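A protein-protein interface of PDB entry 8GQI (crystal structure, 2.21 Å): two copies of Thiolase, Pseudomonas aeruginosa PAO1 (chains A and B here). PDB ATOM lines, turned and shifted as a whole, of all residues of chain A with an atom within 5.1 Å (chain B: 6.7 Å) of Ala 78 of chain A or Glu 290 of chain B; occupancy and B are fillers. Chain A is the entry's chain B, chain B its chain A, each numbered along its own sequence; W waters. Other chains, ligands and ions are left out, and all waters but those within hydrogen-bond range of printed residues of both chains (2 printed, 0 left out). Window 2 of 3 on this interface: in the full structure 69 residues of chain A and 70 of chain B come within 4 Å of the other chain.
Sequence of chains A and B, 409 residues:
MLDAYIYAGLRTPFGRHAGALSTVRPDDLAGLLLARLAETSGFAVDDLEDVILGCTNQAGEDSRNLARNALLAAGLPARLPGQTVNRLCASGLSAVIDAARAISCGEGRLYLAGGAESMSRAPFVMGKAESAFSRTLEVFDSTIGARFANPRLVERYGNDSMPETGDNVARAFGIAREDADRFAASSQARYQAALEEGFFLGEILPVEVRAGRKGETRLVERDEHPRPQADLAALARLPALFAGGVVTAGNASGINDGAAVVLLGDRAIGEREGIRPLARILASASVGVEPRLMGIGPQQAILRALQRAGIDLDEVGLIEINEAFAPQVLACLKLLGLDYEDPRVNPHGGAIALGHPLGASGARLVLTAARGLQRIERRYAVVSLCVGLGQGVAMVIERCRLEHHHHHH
N of Gly 288 of chain B is in hydrogen-bond range of O of Arg 79 of chain A, 3.0 Å away. The backbone carbonyl oxygen (O) of Val 289 of chain B lies within hydrogen-bond range of the guanidinium group (NH2) of Arg 68 of chain A (3.0 Å). The backbone NH (N) of Val 289 of chain B lies within hydrogen-bond range of the backbone carbonyl oxygen (O) of Ala 78 of chain A (3.4 Å). The backbone carbonyl oxygen (O) of Leu 389 of chain B lies within hydrogen-bond range of the guanidinium group (NH2) of Arg 68 of chain A (2.8 Å). O of Gly 390 of chain B lies within hydrogen-bond range of NH2 of Arg 68 of chain A (3.0 Å).
The backbone carbonyl oxygen of Gly 390 of chain B lies within hydrogen-bond range of the backbone NH of Val 289 of chain B (2.8 Å). The guanidinium group (NH1) of Arg 68 of chain A sits at hydrogen-bond distance from the backbone carbonyl oxygen (O) of Ala 78 of chain A (2.8 Å). NH1 of Arg 68 of chain A sits at hydrogen-bond distance from O of Leu 80 of chain A (2.7 Å).
Among the printed residues, merely in contact across the chains: Arg 68 of chain A with Gln 391 of chain B (3.6 Å), Leu 72 of chain A with Arg 156 of chain B (3.5 Å), Leu 72 of chain A with Tyr 157 of chain B (3.6 Å), Leu 72 of chain A with Leu 389 of chain B (3.98 Å), Ala 78 of chain A with Gly 288 of chain B (3.2 Å) and Ala 78 of chain A with Glu 290 of chain B (3.97 Å).
Of the printed residues of chain B, Arg 68 of chain A touches Val 289, Leu 389, Gly 390 and Gln 391. Ala 78 of chain A touches three residues of chain B. Of the printed residues of chain B, Arg 79 of chain A touches Gly 288. Of the printed residues of chain A, Val 289 of chain B touches Arg 68 (3.0 Å) and Ala 78 (3.4 Å). Glu 290 of chain B touches just one residue of chain A: Ala 78 (3.97 Å). Of the printed residues of chain A, Leu 389 of chain B touches Arg 68 (2.8 Å) and Leu 72 (3.98 Å). The nearest residue of chain B that does not touch Ala 78 of chain A is Tyr 157 of chain B (4.03 Å). The nearest printed residue of chain A that does not touch Glu 290 of chain B is Arg 68 of chain A (5.2 Å). The nearest printed residue of chain A that does not touch Tyr 157 of chain B is Ala 78 of chain A (4.03 Å).
Printed residues of chain A that touch a printed residue of chain B: Arg 68, Leu 72, Ala 78 and Arg 79. Hydrophobic or aromatic side chains of chain A that line the printed part of chain B: Leu 72 and Ala 78. Among the printed residues, 11 pairs touch across the chains. Among the printed residues, no Asp or Glu carboxylate lies within 4 Å of a Lys or Arg side-chain nitrogen of the other chain.
No position is printed for both chains. Of the 11 pairs that touch across the chains among the printed residues, none has its exchanged pair printed and touching as well.
Water W2 lies within hydrogen-bond range of the backbone carbonyl oxygen (O) of Leu 72 of chain A (2.6 Å), the backbone carbonyl oxygen (O) of Leu 76 of chain A (2.7 Å) and the side-chain hydroxyl (OH) of Tyr 157 of chain B (2.8 Å). Water W1 lies within hydrogen-bond range of the side-chain hydroxyl (OH) of Tyr 157 of chain B (2.7 Å) and the backbone NH (N) of Ala 78 of chain A (3.0 Å).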
ATOM      1  N   ARG A  68      14.723 -21.757 -15.227  1.00  0.00           N
ATOM      2  CA  ARG A  68      16.126 -21.320 -15.442  1.00  0.00           C
ATOM      3  C   ARG A  68      17.004 -22.534 -15.795  1.00  0.00           C
ATOM      4  O   ARG A  68      17.851 -22.410 -16.682  1.00  0.00           O
ATOM      5  CB  ARG A  68      16.610 -20.589 -14.195  1.00  0.00           C
ATOM      6  CG  ARG A  68      18.055 -20.156 -14.233  1.00  0.00           C
ATOM      7  CD  ARG A  68      18.323 -19.166 -15.355  1.00  0.00           C
ATOM      8  NE  ARG A  68      19.697 -18.696 -15.292  1.00  0.00           N
ATOM      9  CZ  ARG A  68      20.266 -17.868 -16.148  1.00  0.00           C
ATOM     10  NH1 ARG A  68      19.551 -17.359 -17.147  1.00  0.00           N
ATOM     11  NH2 ARG A  68      21.551 -17.542 -15.988  1.00  0.00           N
ATOM     12  N   LEU A  72      18.879 -22.971 -19.516  1.00  0.00           N
ATOM     13  CA  LEU A  72      20.370 -23.030 -19.619  1.00  0.00           C
ATOM     14  C   LEU A  72      20.788 -24.350 -20.301  1.00  0.00           C
ATOM     15  O   LEU A  72      21.702 -24.327 -21.141  1.00  0.00           O
ATOM     16  CB  LEU A  72      21.013 -22.927 -18.232  1.00  0.00           C
ATOM     17  CG  LEU A  72      20.961 -21.555 -17.559  1.00  0.00           C
ATOM     18  CD1 LEU A  72      21.415 -21.673 -16.122  1.00  0.00           C
ATOM     19  CD2 LEU A  72      21.801 -20.523 -18.275  1.00  0.00           C
ATOM     20  N   LEU A  76      19.629 -21.890 -24.460  1.00  0.00           N
ATOM     21  CA  LEU A  76      19.170 -20.477 -24.517  1.00  0.00           C
ATOM     22  C   LEU A  76      20.225 -19.629 -23.813  1.00  0.00           C
ATOM     23  O   LEU A  76      21.017 -20.140 -23.015  1.00  0.00           O
ATOM     24  CB  LEU A  76      17.783 -20.310 -23.895  1.00  0.00           C
ATOM     25  CG  LEU A  76      16.616 -20.772 -24.771  1.00  0.00           C
ATOM     26  CD1 LEU A  76      16.575 -22.277 -24.896  1.00  0.00           C
ATOM     27  CD2 LEU A  76      15.294 -20.303 -24.209  1.00  0.00           C
ATOM     28  N   PRO A  77      20.322 -18.313 -24.080  1.00  0.00           N
ATOM     29  CA  PRO A  77      21.368 -17.497 -23.451  1.00  0.00           C
ATOM     30  C   PRO A  77      21.230 -17.292 -21.926  1.00  0.00           C
ATOM     31  O   PRO A  77      20.126 -17.229 -21.388  1.00  0.00           O
ATOM     32  CB  PRO A  77      21.252 -16.135 -24.163  1.00  0.00           C
ATOM     33  CG  PRO A  77      20.443 -16.430 -25.397  1.00  0.00           C
ATOM     34  CD  PRO A  77      19.490 -17.542 -25.008  1.00  0.00           C
ATOM     35  N   ALA A  78      22.372 -17.148 -21.265  1.00  0.00           N
ATOM     36  CA  ALA A  78      22.518 -16.950 -19.811  1.00  0.00           C
ATOM     37  C   ALA A  78      21.862 -15.632 -19.392  1.00  0.00           C
ATOM     38  O   ALA A  78      21.414 -15.582 -18.223  1.00  0.00           O
ATOM     39  CB  ALA A  78      23.990 -16.939 -19.448  1.00  0.00           C
ATOM     40  N   ARG A  79      21.754 -14.662 -20.312  1.00  0.00           N
ATOM     41  CA  ARG A  79      21.101 -13.356 -20.055  1.00  0.00           C
ATOM     42  C   ARG A  79      19.582 -13.547 -19.832  1.00  0.00           C
ATOM     43  O   ARG A  79      18.943 -12.605 -19.401  1.00  0.00           O
ATOM     44  CB  ARG A  79      21.398 -12.355 -21.184  1.00  0.00           C
ATOM     45  CG  ARG A  79      20.584 -12.595 -22.454  1.00  0.00           C
ATOM     46  CD  ARG A  79      20.380 -11.392 -23.376  1.00  0.00           C
ATOM     47  NE  ARG A  79      21.638 -10.855 -23.913  1.00  0.00           N
ATOM     48  CZ  ARG A  79      22.339 -11.356 -24.941  1.00  0.00           C
ATOM     49  NH1 ARG A  79      23.466 -10.760 -25.305  1.00  0.00           N
ATOM     50  NH2 ARG A  79      21.930 -12.436 -25.598  1.00  0.00           N
ATOM     51  N   LEU A  80      18.994 -14.692 -20.159  1.00  0.00           N
ATOM     52  CA  LEU A  80      17.516 -14.852 -20.133  1.00  0.00           C
ATOM     53  C   LEU A  80      17.039 -15.387 -18.782  1.00  0.00           C
ATOM     54  O   LEU A  80      17.338 -16.516 -18.412  1.00  0.00           O
ATOM     55  CB  LEU A  80      17.109 -15.782 -21.272  1.00  0.00           C
ATOM     56  CG  LEU A  80      15.604 -16.060 -21.339  1.00  0.00           C
ATOM     57  CD1 LEU A  80      14.825 -14.766 -21.606  1.00  0.00           C
ATOM     58  CD2 LEU A  80      15.307 -17.095 -22.400  1.00  0.00           C
ATOM     59  N   ARG B 156      28.403 -26.727 -19.674  1.00  0.00           N
ATOM     60  CA  ARG B 156      28.433 -25.328 -20.179  1.00  0.00           C
ATOM     61  C   ARG B 156      28.883 -24.377 -19.069  1.00  0.00           C
ATOM     62  O   ARG B 156      29.639 -23.446 -19.409  1.00  0.00           O
ATOM     63  CB  ARG B 156      27.077 -24.824 -20.689  1.00  0.00           C
ATOM     64  CG  ARG B 156      26.457 -25.636 -21.821  1.00  0.00           C
ATOM     65  CD  ARG B 156      24.986 -25.302 -22.038  1.00  0.00           C
ATOM     66  NE  ARG B 156      24.285 -26.150 -22.999  1.00  0.00           N
ATOM     67  CZ  ARG B 156      24.335 -26.013 -24.316  1.00  0.00           C
ATOM     68  NH1 ARG B 156      25.091 -25.077 -24.871  1.00  0.00           N
ATOM     69  NH2 ARG B 156      23.630 -26.825 -25.083  1.00  0.00           N
ATOM     70  N   TYR B 157      28.416 -24.566 -17.816  1.00  0.00           N
ATOM     71  CA  TYR B 157      28.416 -23.483 -16.785  1.00  0.00           C
ATOM     72  C   TYR B 157      29.225 -23.833 -15.528  1.00  0.00           C
ATOM     73  O   TYR B 157      29.525 -22.884 -14.790  1.00  0.00           O
ATOM     74  CB  TYR B 157      26.979 -23.048 -16.479  1.00  0.00           C
ATOM     75  CG  TYR B 157      26.328 -22.393 -17.667  1.00  0.00           C
ATOM     76  CD1 TYR B 157      26.851 -21.224 -18.211  1.00  0.00           C
ATOM     77  CD2 TYR B 157      25.237 -22.970 -18.296  1.00  0.00           C
ATOM     78  CE1 TYR B 157      26.270 -20.613 -19.314  1.00  0.00           C
ATOM     79  CE2 TYR B 157      24.645 -22.370 -19.398  1.00  0.00           C
ATOM     80  CZ  TYR B 157      25.158 -21.186 -19.905  1.00  0.00           C
ATOM     81  OH  TYR B 157      24.590 -20.611 -21.006  1.00  0.00           O
ATOM     82  N   VAL B 287      16.916  -9.900 -14.826  1.00  0.00           N
ATOM     83  CA  VAL B 287      18.034 -10.166 -15.772  1.00  0.00           C
ATOM     84  C   VAL B 287      18.665 -11.528 -15.426  1.00  0.00           C
ATOM     85  O   VAL B 287      18.593 -11.959 -14.232  1.00  0.00           O
ATOM     86  CB  VAL B 287      19.091  -9.049 -15.730  1.00  0.00           C
ATOM     87  CG1 VAL B 287      18.477  -7.687 -15.985  1.00  0.00           C
ATOM     88  CG2 VAL B 287      19.862  -9.042 -14.422  1.00  0.00           C
ATOM     89  N   GLY B 288      19.264 -12.167 -16.439  1.00  0.00           N
ATOM     90  CA  GLY B 288      20.134 -13.333 -16.268  1.00  0.00           C
ATOM     91  C   GLY B 288      21.567 -12.877 -16.397  1.00  0.00           C
ATOM     92  O   GLY B 288      21.822 -11.930 -17.136  1.00  0.00           O
ATOM     93  N   VAL B 289      22.485 -13.517 -15.690  1.00  0.00           N
ATOM     94  CA  VAL B 289      23.949 -13.325 -15.888  1.00  0.00           C
ATOM     95  C   VAL B 289      24.600 -14.714 -15.904  1.00  0.00           C
ATOM     96  O   VAL B 289      23.876 -15.739 -15.720  1.00  0.00           O
ATOM     97  CB  VAL B 289      24.532 -12.425 -14.780  1.00  0.00           C
ATOM     98  CG1 VAL B 289      23.976 -11.018 -14.836  1.00  0.00           C
ATOM     99  CG2 VAL B 289      24.293 -13.017 -13.402  1.00  0.00           C
ATOM    100  N   GLU B 290      25.918 -14.752 -16.104  1.00  0.00           N
ATOM    101  CA  GLU B 290      26.717 -15.996 -16.012  1.00  0.00           C
ATOM    102  C   GLU B 290      26.482 -16.591 -14.625  1.00  0.00           C
ATOM    103  O   GLU B 290      26.618 -15.904 -13.609  1.00  0.00           O
ATOM    104  CB  GLU B 290      28.204 -15.717 -16.289  1.00  0.00           C
ATOM    105  CG  GLU B 290      28.509 -15.308 -17.729  1.00  0.00           C
ATOM    106  CD  GLU B 290      28.184 -16.342 -18.809  1.00  0.00           C
ATOM    107  OE1 GLU B 290      28.301 -17.572 -18.527  1.00  0.00           O
ATOM    108  OE2 GLU B 290      27.795 -15.924 -19.929  1.00  0.00           O
ATOM    109  N   PRO B 291      26.075 -17.875 -14.535  1.00  0.00           N
ATOM    110  CA  PRO B 291      25.909 -18.553 -13.243  1.00  0.00           C
ATOM    111  C   PRO B 291      27.082 -18.381 -12.256  1.00  0.00           C
ATOM    112  O   PRO B 291      26.856 -18.193 -11.052  1.00  0.00           O
ATOM    113  CB  PRO B 291      25.736 -20.009 -13.700  1.00  0.00           C
ATOM    114  CG  PRO B 291      24.961 -19.865 -14.991  1.00  0.00           C
ATOM    115  CD  PRO B 291      25.663 -18.709 -15.673  1.00  0.00           C
ATOM    116  N   ARG B 292      28.308 -18.403 -12.772  1.00  0.00           N
ATOM    117  CA  ARG B 292      29.536 -18.343 -11.950  1.00  0.00           C
ATOM    118  C   ARG B 292      29.691 -16.947 -11.331  1.00  0.00           C
ATOM    119  O   ARG B 292      30.430 -16.873 -10.370  1.00  0.00           O
ATOM    120  CB  ARG B 292      30.762 -18.780 -12.772  1.00  0.00           C
ATOM    121  CG  ARG B 292      31.240 -17.777 -13.811  1.00  0.00           C
ATOM    122  CD  ARG B 292      32.447 -18.296 -14.596  1.00  0.00           C
ATOM    123  NE  ARG B 292      33.580 -18.537 -13.695  1.00  0.00           N
ATOM    124  CZ  ARG B 292      34.421 -17.601 -13.239  1.00  0.00           C
ATOM    125  NH1 ARG B 292      34.298 -16.338 -13.616  1.00  0.00           N
ATOM    126  NH2 ARG B 292      35.391 -17.937 -12.402  1.00  0.00           N
ATOM    127  N   LEU B 293      29.057 -15.886 -11.878  1.00  0.00           N
ATOM    128  CA  LEU B 293      29.136 -14.492 -11.343  1.00  0.00           C
ATOM    129  C   LEU B 293      27.763 -13.998 -10.907  1.00  0.00           C
ATOM    130  O   LEU B 293      27.489 -12.779 -11.079  1.00  0.00           O
ATOM    131  CB  LEU B 293      29.664 -13.557 -12.425  1.00  0.00           C
ATOM    132  CG  LEU B 293      31.029 -13.938 -12.979  1.00  0.00           C
ATOM    133  CD1 LEU B 293      31.352 -13.063 -14.184  1.00  0.00           C
ATOM    134  CD2 LEU B 293      32.079 -13.827 -11.894  1.00  0.00           C
ATOM    135  N   MET B 294      26.925 -14.906 -10.416  1.00  0.00           N
ATOM    136  CA  MET B 294      25.481 -14.658 -10.168  1.00  0.00           C
ATOM    137  C   MET B 294      25.289 -13.399  -9.300  1.00  0.00           C
ATOM    138  O   MET B 294      24.224 -12.739  -9.429  1.00  0.00           O
ATOM    139  CB  MET B 294      24.850 -15.885  -9.499  1.00  0.00           C
ATOM    140  CG  MET B 294      25.374 -16.145  -8.089  1.00  0.00           C
ATOM    141  SD  MET B 294      24.246 -15.508  -6.803  1.00  0.00           S
ATOM    142  CE  MET B 294      25.415 -15.276  -5.467  1.00  0.00           C
ATOM    143  N   GLY B 295      26.273 -13.094  -8.446  1.00  0.00           N
ATOM    144  CA  GLY B 295      26.226 -12.040  -7.413  1.00  0.00           C
ATOM    145  C   GLY B 295      26.162 -10.631  -7.988  1.00  0.00           C
ATOM    146  O   GLY B 295      25.741  -9.724  -7.221  1.00  0.00           O
ATOM    147  N   ILE B 296      26.534 -10.429  -9.259  1.00  0.00           N
ATOM    148  CA  ILE B 296      26.421  -9.087  -9.916  1.00  0.00           C
ATOM    149  C   ILE B 296      25.079  -8.935 -10.650  1.00  0.00           C
ATOM    150  O   ILE B 296      24.843  -7.799 -11.207  1.00  0.00           O
ATOM    151  CB  ILE B 296      27.661  -8.774 -10.787  1.00  0.00           C
ATOM    152  CG1 ILE B 296      27.943  -9.844 -11.837  1.00  0.00           C
ATOM    153  CG2 ILE B 296      28.862  -8.545  -9.872  1.00  0.00           C
ATOM    154  CD1 ILE B 296      26.819 -10.039 -12.833  1.00  0.00           C
ATOM    155  N   LEU B 389      22.303 -19.514  -9.972  1.00  0.00           N
ATOM    156  CA  LEU B 389      22.293 -19.888 -11.413  1.00  0.00           C
ATOM    157  C   LEU B 389      22.236 -18.612 -12.272  1.00  0.00           C
ATOM    158  O   LEU B 389      22.078 -18.728 -13.521  1.00  0.00           O
ATOM    159  CB  LEU B 389      21.153 -20.868 -11.732  1.00  0.00           C
ATOM    160  CG  LEU B 389      21.413 -22.346 -11.439  1.00  0.00           C
ATOM    161  CD1 LEU B 389      22.759 -22.810 -11.981  1.00  0.00           C
ATOM    162  CD2 LEU B 389      21.369 -22.631  -9.956  1.00  0.00           C
ATOM    163  N   GLY B 390      22.424 -17.443 -11.653  1.00  0.00           N
ATOM    164  CA  GLY B 390      22.744 -16.173 -12.346  1.00  0.00           C
ATOM    165  C   GLY B 390      21.500 -15.405 -12.748  1.00  0.00           C
ATOM    166  O   GLY B 390      21.212 -15.310 -13.951  1.00  0.00           O
ATOM    167  N   GLN B 391      20.815 -14.817 -11.781  1.00  0.00           N
ATOM    168  CA  GLN B 391      19.761 -13.808 -12.060  1.00  0.00           C
ATOM    169  C   GLN B 391      19.873 -12.653 -11.065  1.00  0.00           C
ATOM    170  O   GLN B 391      20.530 -12.824 -10.006  1.00  0.00           O
ATOM    171  CB  GLN B 391      18.358 -14.416 -12.017  1.00  0.00           C
ATOM    172  CG  GLN B 391      18.240 -15.751 -12.743  1.00  0.00           C
ATOM    173  CD  GLN B 391      16.810 -16.229 -12.863  1.00  0.00           C
ATOM    174  OE1 GLN B 391      16.489 -17.381 -12.565  1.00  0.00           O
ATOM    175  NE2 GLN B 391      15.924 -15.340 -13.293  1.00  0.00           N
HETATM  176  O   HOH W   1      24.908 -18.273 -22.277  1.00  0.00           O
HETATM  177  O   HOH W   2      22.625 -22.196 -22.214  1.00  0.00           O
